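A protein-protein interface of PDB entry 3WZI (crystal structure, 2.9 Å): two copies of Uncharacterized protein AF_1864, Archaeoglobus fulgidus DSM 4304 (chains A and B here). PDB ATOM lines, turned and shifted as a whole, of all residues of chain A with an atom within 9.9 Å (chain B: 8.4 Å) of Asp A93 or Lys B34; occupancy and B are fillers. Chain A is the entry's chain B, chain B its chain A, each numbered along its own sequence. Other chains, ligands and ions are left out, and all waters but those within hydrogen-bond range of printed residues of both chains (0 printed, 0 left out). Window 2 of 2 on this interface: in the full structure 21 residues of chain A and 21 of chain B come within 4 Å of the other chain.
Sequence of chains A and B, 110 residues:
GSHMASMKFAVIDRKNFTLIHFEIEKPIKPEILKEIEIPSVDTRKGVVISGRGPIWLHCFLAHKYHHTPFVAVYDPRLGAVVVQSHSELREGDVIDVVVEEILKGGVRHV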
ATOM      1  N   VAL A  48     -22.668  17.578 -20.916  1.00  0.00           N
ATOM      2  CA  VAL A  48     -23.182  18.557 -19.982  1.00  0.00           C
ATOM      3  C   VAL A  48     -23.592  17.798 -18.754  1.00  0.00           C
ATOM      4  O   VAL A  48     -24.264  16.781 -18.833  1.00  0.00           O
ATOM      5  CB  VAL A  48     -24.407  19.281 -20.582  1.00  0.00           C
ATOM      6  CG1 VAL A  48     -25.097  20.134 -19.580  1.00  0.00           C
ATOM      7  CG2 VAL A  48     -23.997  20.121 -21.762  1.00  0.00           C
ATOM      8  N   PHE A  70     -15.651  18.465 -24.619  1.00  0.00           N
ATOM      9  CA  PHE A  70     -15.815  19.500 -23.645  1.00  0.00           C
ATOM     10  C   PHE A  70     -16.642  19.075 -22.504  1.00  0.00           C
ATOM     11  O   PHE A  70     -17.352  18.106 -22.609  1.00  0.00           O
ATOM     12  CB  PHE A  70     -16.464  20.734 -24.248  1.00  0.00           C
ATOM     13  CG  PHE A  70     -17.851  20.528 -24.747  1.00  0.00           C
ATOM     14  CD1 PHE A  70     -18.936  20.490 -23.894  1.00  0.00           C
ATOM     15  CD2 PHE A  70     -18.100  20.547 -26.093  1.00  0.00           C
ATOM     16  CE1 PHE A  70     -20.261  20.417 -24.408  1.00  0.00           C
ATOM     17  CE2 PHE A  70     -19.405  20.457 -26.605  1.00  0.00           C
ATOM     18  CZ  PHE A  70     -20.477  20.385 -25.781  1.00  0.00           C
ATOM     19  N   VAL A  71     -16.563  19.825 -21.418  1.00  0.00           N
ATOM     20  CA  VAL A  71     -17.430  19.603 -20.312  1.00  0.00           C
ATOM     21  C   VAL A  71     -18.091  20.967 -19.894  1.00  0.00           C
ATOM     22  O   VAL A  71     -17.450  22.013 -19.719  1.00  0.00           O
ATOM     23  CB  VAL A  71     -16.653  19.073 -19.139  1.00  0.00           C
ATOM     24  CG1 VAL A  71     -17.632  18.593 -18.082  1.00  0.00           C
ATOM     25  CG2 VAL A  71     -15.724  17.941 -19.528  1.00  0.00           C
ATOM     26  N   ALA A  72     -19.382  20.936 -19.711  1.00  0.00           N
ATOM     27  CA  ALA A  72     -20.095  22.065 -19.320  1.00  0.00           C
ATOM     28  C   ALA A  72     -20.863  21.669 -18.117  1.00  0.00           C
ATOM     29  O   ALA A  72     -21.364  20.590 -17.995  1.00  0.00           O
ATOM     30  CB  ALA A  72     -21.032  22.460 -20.422  1.00  0.00           C
ATOM     31  N   VAL A  73     -21.031  22.612 -17.228  1.00  0.00           N
ATOM     32  CA  VAL A  73     -21.651  22.357 -15.975  1.00  0.00           C
ATOM     33  C   VAL A  73     -22.895  23.154 -15.971  1.00  0.00           C
ATOM     34  O   VAL A  73     -22.834  24.338 -16.232  1.00  0.00           O
ATOM     35  CB  VAL A  73     -20.760  22.842 -14.888  1.00  0.00           C
ATOM     36  CG1 VAL A  73     -21.524  22.813 -13.600  1.00  0.00           C
ATOM     37  CG2 VAL A  73     -19.555  21.925 -14.807  1.00  0.00           C
ATOM     38  N   TYR A  74     -24.026  22.521 -15.693  1.00  0.00           N
ATOM     39  CA  TYR A  74     -25.279  23.199 -15.793  1.00  0.00           C
ATOM     40  C   TYR A  74     -25.502  24.142 -14.641  1.00  0.00           C
ATOM     41  O   TYR A  74     -25.059  23.895 -13.536  1.00  0.00           O
ATOM     42  CB  TYR A  74     -26.430  22.270 -15.848  1.00  0.00           C
ATOM     43  CG  TYR A  74     -27.744  22.939 -16.146  1.00  0.00           C
ATOM     44  CD1 TYR A  74     -28.007  23.508 -17.399  1.00  0.00           C
ATOM     45  CD2 TYR A  74     -28.740  23.030 -15.171  1.00  0.00           C
ATOM     46  CE1 TYR A  74     -29.241  24.116 -17.661  1.00  0.00           C
ATOM     47  CE2 TYR A  74     -29.983  23.605 -15.432  1.00  0.00           C
ATOM     48  CZ  TYR A  74     -30.224  24.137 -16.656  1.00  0.00           C
ATOM     49  OH  TYR A  74     -31.448  24.635 -16.912  1.00  0.00           O
ATOM     50  N   ASP A  75     -26.193  25.227 -14.970  1.00  0.00           N
ATOM     51  CA  ASP A  75     -26.626  26.249 -14.035  1.00  0.00           C
ATOM     52  C   ASP A  75     -28.008  26.785 -14.465  1.00  0.00           C
ATOM     53  O   ASP A  75     -28.125  27.431 -15.522  1.00  0.00           O
ATOM     54  CB  ASP A  75     -25.595  27.368 -14.034  1.00  0.00           C
ATOM     55  CG  ASP A  75     -25.963  28.480 -13.130  1.00  0.00           C
ATOM     56  OD1 ASP A  75     -27.168  28.681 -12.896  1.00  0.00           O
ATOM     57  OD2 ASP A  75     -25.033  29.128 -12.629  1.00  0.00           O
ATOM     58  N   LEU A  78     -28.410  30.217 -16.047  1.00  0.00           N
ATOM     59  CA  LEU A  78     -27.663  30.621 -17.245  1.00  0.00           C
ATOM     60  C   LEU A  78     -27.714  29.686 -18.399  1.00  0.00           C
ATOM     61  O   LEU A  78     -27.765  30.079 -19.561  1.00  0.00           O
ATOM     62  CB  LEU A  78     -26.202  30.718 -16.870  1.00  0.00           C
ATOM     63  CG  LEU A  78     -25.983  31.699 -15.729  1.00  0.00           C
ATOM     64  CD1 LEU A  78     -24.662  31.384 -15.064  1.00  0.00           C
ATOM     65  CD2 LEU A  78     -26.022  33.117 -16.245  1.00  0.00           C
ATOM     66  N   GLY A  79     -27.588  28.421 -18.078  1.00  0.00           N
ATOM     67  CA  GLY A  79     -27.451  27.371 -19.096  1.00  0.00           C
ATOM     68  C   GLY A  79     -26.245  26.543 -18.750  1.00  0.00           C
ATOM     69  O   GLY A  79     -25.912  26.366 -17.569  1.00  0.00           O
ATOM     70  N   ALA A  80     -25.573  26.031 -19.765  1.00  0.00           N
ATOM     71  CA  ALA A  80     -24.513  25.103 -19.484  1.00  0.00           C
ATOM     72  C   ALA A  80     -23.187  25.796 -19.715  1.00  0.00           C
ATOM     73  O   ALA A  80     -22.901  26.232 -20.848  1.00  0.00           O
ATOM     74  CB  ALA A  80     -24.661  23.879 -20.340  1.00  0.00           C
ATOM     75  N   VAL A  81     -22.404  25.939 -18.638  1.00  0.00           N
ATOM     76  CA  VAL A  81     -21.160  26.689 -18.714  1.00  0.00           C
ATOM     77  C   VAL A  81     -20.027  25.722 -19.088  1.00  0.00           C
ATOM     78  O   VAL A  81     -19.603  24.963 -18.283  1.00  0.00           O
ATOM     79  CB  VAL A  81     -20.807  27.367 -17.366  1.00  0.00           C
ATOM     80  CG1 VAL A  81     -19.481  28.087 -17.432  1.00  0.00           C
ATOM     81  CG2 VAL A  81     -21.852  28.370 -17.003  1.00  0.00           C
ATOM     82  N   VAL A  82     -19.448  25.893 -20.251  1.00  0.00           N
ATOM     83  CA  VAL A  82     -18.230  25.224 -20.531  1.00  0.00           C
ATOM     84  C   VAL A  82     -17.145  25.475 -19.457  1.00  0.00           C
ATOM     85  O   VAL A  82     -16.855  26.572 -19.145  1.00  0.00           O
ATOM     86  CB  VAL A  82     -17.727  25.601 -21.929  1.00  0.00           C
ATOM     87  CG1 VAL A  82     -16.501  24.761 -22.291  1.00  0.00           C
ATOM     88  CG2 VAL A  82     -18.812  25.334 -22.953  1.00  0.00           C
ATOM     89  N   VAL A  83     -16.488  24.421 -18.976  1.00  0.00           N
ATOM     90  CA  VAL A  83     -15.387  24.537 -18.007  1.00  0.00           C
ATOM     91  C   VAL A  83     -14.139  23.789 -18.412  1.00  0.00           C
ATOM     92  O   VAL A  83     -13.083  23.859 -17.761  1.00  0.00           O
ATOM     93  CB  VAL A  83     -15.781  23.980 -16.654  1.00  0.00           C
ATOM     94  CG1 VAL A  83     -17.029  24.736 -16.101  1.00  0.00           C
ATOM     95  CG2 VAL A  83     -16.051  22.499 -16.816  1.00  0.00           C
ATOM     96  N   GLN A  84     -14.213  23.083 -19.509  1.00  0.00           N
ATOM     97  CA  GLN A  84     -13.009  22.433 -20.090  1.00  0.00           C
ATOM     98  C   GLN A  84     -13.305  22.381 -21.549  1.00  0.00           C
ATOM     99  O   GLN A  84     -14.446  22.047 -21.916  1.00  0.00           O
ATOM    100  CB  GLN A  84     -12.881  20.989 -19.620  1.00  0.00           C
ATOM    101  CG  GLN A  84     -12.783  20.775 -18.148  1.00  0.00           C
ATOM    102  CD  GLN A  84     -12.940  19.343 -17.738  1.00  0.00           C
ATOM    103  OE1 GLN A  84     -12.268  18.480 -18.281  1.00  0.00           O
ATOM    104  NE2 GLN A  84     -13.771  19.090 -16.727  1.00  0.00           N
ATOM    105  N   SER A  85     -12.322  22.603 -22.403  1.00  0.00           N
ATOM    106  CA  SER A  85     -12.573  22.251 -23.795  1.00  0.00           C
ATOM    107  C   SER A  85     -11.368  21.865 -24.696  1.00  0.00           C
ATOM    108  O   SER A  85     -10.245  22.228 -24.431  1.00  0.00           O
ATOM    109  CB  SER A  85     -13.411  23.299 -24.451  1.00  0.00           C
ATOM    110  OG  SER A  85     -13.203  23.288 -25.874  1.00  0.00           O
ATOM    111  N   SER A  87     -12.757  21.301 -28.127  1.00  0.00           N
ATOM    112  CA  SER A  87     -13.490  21.582 -29.338  1.00  0.00           C
ATOM    113  C   SER A  87     -13.472  23.104 -29.585  1.00  0.00           C
ATOM    114  O   SER A  87     -12.703  23.791 -28.961  1.00  0.00           O
ATOM    115  CB  SER A  87     -14.907  21.106 -29.157  1.00  0.00           C
ATOM    116  OG  SER A  87     -15.536  21.735 -28.034  1.00  0.00           O
ATOM    117  N   GLU A  88     -14.346  23.573 -30.484  1.00  0.00           N
ATOM    118  CA  GLU A  88     -14.562  24.980 -30.810  1.00  0.00           C
ATOM    119  C   GLU A  88     -14.973  25.740 -29.576  1.00  0.00           C
ATOM    120  O   GLU A  88     -14.460  26.805 -29.326  1.00  0.00           O
ATOM    121  CB  GLU A  88     -15.662  25.114 -31.878  1.00  0.00           C
ATOM    122  CG  GLU A  88     -15.707  26.512 -32.517  1.00  0.00           C
ATOM    123  CD  GLU A  88     -16.427  26.629 -33.889  1.00  0.00           C
ATOM    124  OE1 GLU A  88     -16.734  25.629 -34.584  1.00  0.00           O
ATOM    125  OE2 GLU A  88     -16.688  27.776 -34.297  1.00  0.00           O
ATOM    126  N   LEU A  89     -15.859  25.177 -28.762  1.00  0.00           N
ATOM    127  CA  LEU A  89     -16.344  25.899 -27.594  1.00  0.00           C
ATOM    128  C   LEU A  89     -15.203  26.296 -26.693  1.00  0.00           C
ATOM    129  O   LEU A  89     -14.292  25.527 -26.515  1.00  0.00           O
ATOM    130  CB  LEU A  89     -17.325  25.048 -26.827  1.00  0.00           C
ATOM    131  CG  LEU A  89     -18.649  24.845 -27.566  1.00  0.00           C
ATOM    132  CD1 LEU A  89     -19.583  23.939 -26.771  1.00  0.00           C
ATOM    133  CD2 LEU A  89     -19.340  26.174 -27.761  1.00  0.00           C
ATOM    134  N   ARG A  90     -15.268  27.508 -26.140  1.00  0.00           N
ATOM    135  CA  ARG A  90     -14.241  28.047 -25.254  1.00  0.00           C
ATOM    136  C   ARG A  90     -14.737  28.060 -23.816  1.00  0.00           C
ATOM    137  O   ARG A  90     -15.921  28.157 -23.556  1.00  0.00           O
ATOM    138  CB  ARG A  90     -13.876  29.479 -25.674  1.00  0.00           C
ATOM    139  CG  ARG A  90     -13.197  29.596 -27.019  1.00  0.00           C
ATOM    140  CD  ARG A  90     -12.666  31.001 -27.262  1.00  0.00           C
ATOM    141  NE  ARG A  90     -12.071  31.144 -28.604  1.00  0.00           N
ATOM    142  CZ  ARG A  90     -11.457  32.243 -29.076  1.00  0.00           C
ATOM    143  NH1 ARG A  90     -11.339  33.331 -28.328  1.00  0.00           N
ATOM    144  NH2 ARG A  90     -10.952  32.251 -30.312  1.00  0.00           N
ATOM    145  N   GLU A  91     -13.828  28.002 -22.865  1.00  0.00           N
ATOM    146  CA  GLU A  91     -14.238  28.042 -21.475  1.00  0.00           C
ATOM    147  C   GLU A  91     -14.954  29.340 -21.181  1.00  0.00           C
ATOM    148  O   GLU A  91     -14.608  30.401 -21.711  1.00  0.00           O
ATOM    149  CB  GLU A  91     -12.999  27.885 -20.621  1.00  0.00           C
ATOM    150  CG  GLU A  91     -12.219  26.617 -20.970  1.00  0.00           C
ATOM    151  CD  GLU A  91     -10.728  26.623 -20.675  1.00  0.00           C
ATOM    152  OE1 GLU A  91     -10.123  27.702 -20.438  1.00  0.00           O
ATOM    153  OE2 GLU A  91     -10.160  25.506 -20.674  1.00  0.00           O
ATOM    154  N   GLY A  92     -15.987  29.292 -20.365  1.00  0.00           N
ATOM    155  CA  GLY A  92     -16.827  30.484 -20.150  1.00  0.00           C
ATOM    156  C   GLY A  92     -17.979  30.566 -21.133  1.00  0.00           C
ATOM    157  O   GLY A  92     -18.946  31.245 -20.852  1.00  0.00           O
ATOM    158  N   ASP A  93     -17.899  29.903 -22.295  1.00  0.00           N
ATOM    159  CA  ASP A  93     -19.018  29.874 -23.248  1.00  0.00           C
ATOM    160  C   ASP A  93     -20.195  29.238 -22.585  1.00  0.00           C
ATOM    161  O   ASP A  93     -20.050  28.504 -21.612  1.00  0.00           O
ATOM    162  CB  ASP A  93     -18.680  29.145 -24.544  1.00  0.00           C
ATOM    163  CG  ASP A  93     -17.850  29.993 -25.491  1.00  0.00           C
ATOM    164  OD1 ASP A  93     -17.576  31.167 -25.130  1.00  0.00           O
ATOM    165  OD2 ASP A  93     -17.415  29.505 -26.567  1.00  0.00           O
ATOM    166  N   VAL A  94     -21.386  29.552 -23.083  1.00  0.00           N
ATOM    167  CA  VAL A  94     -22.632  29.037 -22.503  1.00  0.00           C
ATOM    168  C   VAL A  94     -23.474  28.339 -23.568  1.00  0.00           C
ATOM    169  O   VAL A  94     -23.881  28.941 -24.539  1.00  0.00           O
ATOM    170  CB  VAL A  94     -23.463  30.131 -21.826  1.00  0.00           C
ATOM    171  CG1 VAL A  94     -24.778  29.595 -21.317  1.00  0.00           C
ATOM    172  CG2 VAL A  94     -22.699  30.710 -20.650  1.00  0.00           C
ATOM    173  N   ILE A  95     -23.729  27.057 -23.351  1.00  0.00           N
ATOM    174  CA  ILE A  95     -24.609  26.295 -24.179  1.00  0.00           C
ATOM    175  C   ILE A  95     -26.047  26.491 -23.687  1.00  0.00           C
ATOM    176  O   ILE A  95     -26.376  26.247 -22.504  1.00  0.00           O
ATOM    177  CB  ILE A  95     -24.254  24.774 -24.099  1.00  0.00           C
ATOM    178  CG1 ILE A  95     -22.850  24.538 -24.630  1.00  0.00           C
ATOM    179  CG2 ILE A  95     -25.226  23.950 -24.935  1.00  0.00           C
ATOM    180  CD1 ILE A  95     -22.220  23.255 -24.164  1.00  0.00           C
ATOM    181  N   ASP A  96     -26.914  26.817 -24.636  1.00  0.00           N
ATOM    182  CA  ASP A  96     -28.290  27.070 -24.331  1.00  0.00           C
ATOM    183  C   ASP A  96     -29.146  25.808 -24.259  1.00  0.00           C
ATOM    184  O   ASP A  96     -29.636  25.343 -25.312  1.00  0.00           O
ATOM    185  CB  ASP A  96     -28.860  28.015 -25.400  1.00  0.00           C
ATOM    186  CG  ASP A  96     -30.321  28.352 -25.172  1.00  0.00           C
ATOM    187  OD1 ASP A  96     -30.789  28.272 -23.984  1.00  0.00           O
ATOM    188  OD2 ASP A  96     -30.969  28.674 -26.211  1.00  0.00           O
ATOM    189  N   ALA B   5      -9.650  38.678 -13.477  1.00  0.00           N
ATOM    190  CA  ALA B   5      -9.365  40.151 -13.324  1.00  0.00           C
ATOM    191  C   ALA B   5     -10.023  40.760 -12.025  1.00  0.00           C
ATOM    192  O   ALA B   5      -9.317  41.252 -11.129  1.00  0.00           O
ATOM    193  CB  ALA B   5      -9.778  40.903 -14.605  1.00  0.00           C
ATOM    194  N   LYS B  29     -20.116  36.538 -14.033  1.00  0.00           N
ATOM    195  CA  LYS B  29     -20.571  36.005 -15.300  1.00  0.00           C
ATOM    196  C   LYS B  29     -19.592  34.975 -15.900  1.00  0.00           C
ATOM    197  O   LYS B  29     -18.406  35.058 -15.730  1.00  0.00           O
ATOM    198  CB  LYS B  29     -20.791  37.127 -16.292  1.00  0.00           C
ATOM    199  CG  LYS B  29     -21.882  38.056 -15.871  1.00  0.00           C
ATOM    200  CD  LYS B  29     -22.208  39.068 -16.954  1.00  0.00           C
ATOM    201  CE  LYS B  29     -23.145  40.130 -16.400  1.00  0.00           C
ATOM    202  NZ  LYS B  29     -23.770  40.909 -17.501  1.00  0.00           N
ATOM    203  N   PRO B  30     -20.101  34.006 -16.639  1.00  0.00           N
ATOM    204  CA  PRO B  30     -19.200  32.934 -17.078  1.00  0.00           C
ATOM    205  C   PRO B  30     -18.075  33.444 -17.932  1.00  0.00           C
ATOM    206  O   PRO B  30     -16.990  32.919 -17.899  1.00  0.00           O
ATOM    207  CB  PRO B  30     -20.109  32.029 -17.904  1.00  0.00           C
ATOM    208  CG  PRO B  30     -21.498  32.341 -17.453  1.00  0.00           C
ATOM    209  CD  PRO B  30     -21.486  33.808 -17.091  1.00  0.00           C
ATOM    210  N   GLU B  31     -18.356  34.468 -18.713  1.00  0.00           N
ATOM    211  CA  GLU B  31     -17.363  35.141 -19.533  1.00  0.00           C
ATOM    212  C   GLU B  31     -16.035  35.295 -18.789  1.00  0.00           C
ATOM    213  O   GLU B  31     -14.979  35.069 -19.340  1.00  0.00           O
ATOM    214  CB  GLU B  31     -17.915  36.521 -19.865  1.00  0.00           C
ATOM    215  CG  GLU B  31     -17.121  37.321 -20.889  1.00  0.00           C
ATOM    216  CD  GLU B  31     -17.762  38.682 -21.170  1.00  0.00           C
ATOM    217  OE1 GLU B  31     -18.776  39.019 -20.512  1.00  0.00           O
ATOM    218  OE2 GLU B  31     -17.256  39.425 -22.045  1.00  0.00           O
ATOM    219  N   ILE B  32     -16.106  35.660 -17.515  1.00  0.00           N
ATOM    220  CA  ILE B  32     -14.924  35.830 -16.692  1.00  0.00           C
ATOM    221  C   ILE B  32     -13.938  34.670 -16.777  1.00  0.00           C
ATOM    222  O   ILE B  32     -12.782  34.832 -16.475  1.00  0.00           O
ATOM    223  CB  ILE B  32     -15.299  35.959 -15.210  1.00  0.00           C
ATOM    224  CG1 ILE B  32     -14.149  36.520 -14.415  1.00  0.00           C
ATOM    225  CG2 ILE B  32     -15.627  34.606 -14.579  1.00  0.00           C
ATOM    226  CD1 ILE B  32     -14.540  36.860 -12.993  1.00  0.00           C
ATOM    227  N   LEU B  33     -14.380  33.475 -17.124  1.00  0.00           N
ATOM    228  CA  LEU B  33     -13.450  32.386 -17.127  1.00  0.00           C
ATOM    229  C   LEU B  33     -12.402  32.613 -18.225  1.00  0.00           C
ATOM    230  O   LEU B  33     -11.286  32.151 -18.111  1.00  0.00           O
ATOM    231  CB  LEU B  33     -14.170  31.041 -17.287  1.00  0.00           C
ATOM    232  CG  LEU B  33     -15.184  30.665 -16.219  1.00  0.00           C
ATOM    233  CD1 LEU B  33     -15.935  29.403 -16.633  1.00  0.00           C
ATOM    234  CD2 LEU B  33     -14.526  30.456 -14.889  1.00  0.00           C
ATOM    235  N   LYS B  34     -12.755  33.347 -19.271  1.00  0.00           N
ATOM    236  CA  LYS B  34     -11.815  33.648 -20.355  1.00  0.00           C
ATOM    237  C   LYS B  34     -10.625  34.463 -19.894  1.00  0.00           C
ATOM    238  O   LYS B  34      -9.604  34.467 -20.553  1.00  0.00           O
ATOM    239  CB  LYS B  34     -12.522  34.384 -21.485  1.00  0.00           C
ATOM    240  CG  LYS B  34     -13.639  33.549 -22.076  1.00  0.00           C
ATOM    241  CD  LYS B  34     -14.295  34.195 -23.249  1.00  0.00           C
ATOM    242  CE  LYS B  34     -15.419  33.329 -23.791  1.00  0.00           C
ATOM    243  NZ  LYS B  34     -15.940  34.067 -24.972  1.00  0.00           N
ATOM    244  N   GLU B  35     -10.759  35.113 -18.740  1.00  0.00           N
ATOM    245  CA  GLU B  35      -9.798  36.067 -18.261  1.00  0.00           C
ATOM    246  C   GLU B  35      -9.126  35.705 -16.933  1.00  0.00           C
ATOM    247  O   GLU B  35      -8.162  36.307 -16.591  1.00  0.00           O
ATOM    248  CB  GLU B  35     -10.501  37.420 -18.222  1.00  0.00           C
ATOM    249  CG  GLU B  35     -11.539  37.546 -17.123  1.00  0.00           C
ATOM    250  CD  GLU B  35     -12.300  38.849 -17.194  1.00  0.00           C
ATOM    251  OE1 GLU B  35     -12.048  39.617 -18.131  1.00  0.00           O
ATOM    252  OE2 GLU B  35     -13.145  39.110 -16.313  1.00  0.00           O
ATOM    253  N   ILE B  36      -9.583  34.708 -16.194  1.00  0.00           N
ATOM    254  CA  ILE B  36      -8.924  34.326 -14.932  1.00  0.00           C
ATOM    255  C   ILE B  36      -7.456  33.914 -15.146  1.00  0.00           C
ATOM    256  O   ILE B  36      -7.138  33.079 -16.002  1.00  0.00           O
ATOM    257  CB  ILE B  36      -9.657  33.148 -14.220  1.00  0.00           C
ATOM    258  CG1 ILE B  36     -11.061  33.527 -13.825  1.00  0.00           C
ATOM    259  CG2 ILE B  36      -8.955  32.724 -12.936  1.00  0.00           C
ATOM    260  CD1 ILE B  36     -11.136  34.824 -13.056  1.00  0.00           C
ATOM    261  N   GLU B  37      -6.581  34.472 -14.315  1.00  0.00           N
ATOM    262  CA  GLU B  37      -5.157  34.178 -14.330  1.00  0.00           C
ATOM    263  C   GLU B  37      -4.915  33.435 -13.045  1.00  0.00           C
ATOM    264  O   GLU B  37      -4.883  33.986 -11.950  1.00  0.00           O
ATOM    265  CB  GLU B  37      -4.325  35.453 -14.417  1.00  0.00           C
ATOM    266  CG  GLU B  37      -4.566  36.200 -15.733  1.00  0.00           C
ATOM    267  CD  GLU B  37      -3.774  37.485 -15.900  1.00  0.00           C
ATOM    268  OE1 GLU B  37      -3.083  37.903 -14.940  1.00  0.00           O
ATOM    269  OE2 GLU B  37      -3.845  38.062 -17.011  1.00  0.00           O
ATOM    270  N   TRP B  56     -19.684  25.922 -11.533  1.00  0.00           N
ATOM    271  CA  TRP B  56     -18.813  26.071 -12.692  1.00  0.00           C
ATOM    272  C   TRP B  56     -17.452  26.700 -12.374  1.00  0.00           C
ATOM    273  O   TRP B  56     -16.472  26.478 -13.027  1.00  0.00           O
ATOM    274  CB  TRP B  56     -19.491  26.762 -13.867  1.00  0.00           C
ATOM    275  CG  TRP B  56     -20.235  27.985 -13.604  1.00  0.00           C
ATOM    276  CD1 TRP B  56     -21.587  28.104 -13.334  1.00  0.00           C
ATOM    277  CD2 TRP B  56     -19.719  29.322 -13.633  1.00  0.00           C
ATOM    278  NE1 TRP B  56     -21.913  29.424 -13.202  1.00  0.00           N
ATOM    279  CE2 TRP B  56     -20.791  30.183 -13.392  1.00  0.00           C
ATOM    280  CE3 TRP B  56     -18.462  29.858 -13.884  1.00  0.00           C
ATOM    281  CZ2 TRP B  56     -20.654  31.532 -13.398  1.00  0.00           C
ATOM    282  CZ3 TRP B  56     -18.325  31.173 -13.899  1.00  0.00           C
ATOM    283  CH2 TRP B  56     -19.418  32.021 -13.660  1.00  0.00           C
ATOM    284  N   PHE B  60     -14.132  24.557 -13.119  1.00  0.00           N
ATOM    285  CA  PHE B  60     -13.083  25.195 -13.911  1.00  0.00           C
ATOM    286  C   PHE B  60     -11.743  25.190 -13.211  1.00  0.00           C
ATOM    287  O   PHE B  60     -10.739  24.768 -13.773  1.00  0.00           O
ATOM    288  CB  PHE B  60     -13.484  26.632 -14.174  1.00  0.00           C
ATOM    289  CG  PHE B  60     -12.451  27.406 -14.864  1.00  0.00           C
ATOM    290  CD1 PHE B  60     -12.296  27.308 -16.229  1.00  0.00           C
ATOM    291  CD2 PHE B  60     -11.636  28.271 -14.151  1.00  0.00           C
ATOM    292  CE1 PHE B  60     -11.338  28.067 -16.883  1.00  0.00           C
ATOM    293  CE2 PHE B  60     -10.647  28.995 -14.810  1.00  0.00           C
ATOM    294  CZ  PHE B  60     -10.488  28.873 -16.172  1.00  0.00           C
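The side-chain carboxylate of Asp A75 lies within hydrogen-bond range of the indole nitrogen of Trp B56, at 3.2 Å. The side-chain amino group (NZ) of Lys B34 lies within salt-bridge range of the side-chain carboxylate (OD1) of Asp A93, 3.3 Å away.
The backbone NH (N) of Arg A90 is in hydrogen-bond range of the side-chain carboxylate (OD2) of Asp A93, 3.0 Å away. The backbone carbonyl oxygen (O) of Val A71 lies within hydrogen-bond range of the backbone NH (N) of Val A83, 2.7 Å away. The backbone NH (N) of Val A82 sits at hydrogen-bond distance from the backbone carbonyl oxygen (O) of Asp A93 (3.0 Å). O of Val A82 lies within hydrogen-bond range of N of Gly A92 (3.1 Å). The backbone NH (N) of Val A81 lies within hydrogen-bond range of the backbone carbonyl oxygen (O) of Val A73 (2.9 Å).
Trp B56 touches Leu A78 (NE1 to CD1, 3.9 Å). Leu B33 touches Val A81 (CD1 to CG1, 3.9 Å). Val A81 touches Trp B56 (CG2 to CD1, 3.7 Å). Val A82 touches Leu B33. Phe B60 touches Val A83 (CD1 to O, 3.9 Å). Glu A91 touches Lys B34 (O to CG, 3.3 Å). Glu A91 touches Phe B60. Pro B30 touches Gly A92. Gly A92 touches Glu B31. CD1 of Leu B33 touches N of Gly A92, 3.7 Å away.
Of the printed residues of chain B, Val A82 touches Leu B33 (3.9 Å). Of the printed residues of chain B, Glu A91 touches Lys B34 (3.3 Å) and Phe B60 (3.8 Å). Gly A92 touches just these residues of chain B: Pro B30, Glu B31 and Leu B33. Printed residues of chain B within 4 Å of Asp A93: Lys B34 (3.3 Å). Printed residues of chain B within 4 Å of Val A94: Pro B30 (3.8 Å). Printed residues of chain A within 4 Å of Glu B31: Gly A92 (3.9 Å). Printed residues of chain A within 4 Å of Leu B33: Val A81 (3.9 Å), Val A82 (3.9 Å) and Gly A92 (3.7 Å). Lys B34 touches just these residues of chain A: Glu A91 (3.3 Å) and Asp A93 (3.3 Å). The nearest residue of chain B that does not touch Asp A93 is Pro B30 (5.1 Å).
Of the 12 printed residues of chain B, 6 touch a printed residue of chain A. Printed residues of chain B that touch a printed residue of chain A: Pro B30, Glu B31, Leu B33, Lys B34, Trp B56 and Phe B60. Hydrophobic or aromatic side chains of chain B that line the printed part of chain A: Pro B30, Leu B33, Trp B56 and Phe B60. Hydrophobic or aromatic side chains of chain A that line the printed part of chain B: Leu A78, Val A81, Val A83 and Val A94. Among the printed residues, 14 pairs touch across the chains.
No position is printed for both chains. Of the 14 pairs that touch across the chains among the printed residues, none has its exchanged pair printed and touching as well.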
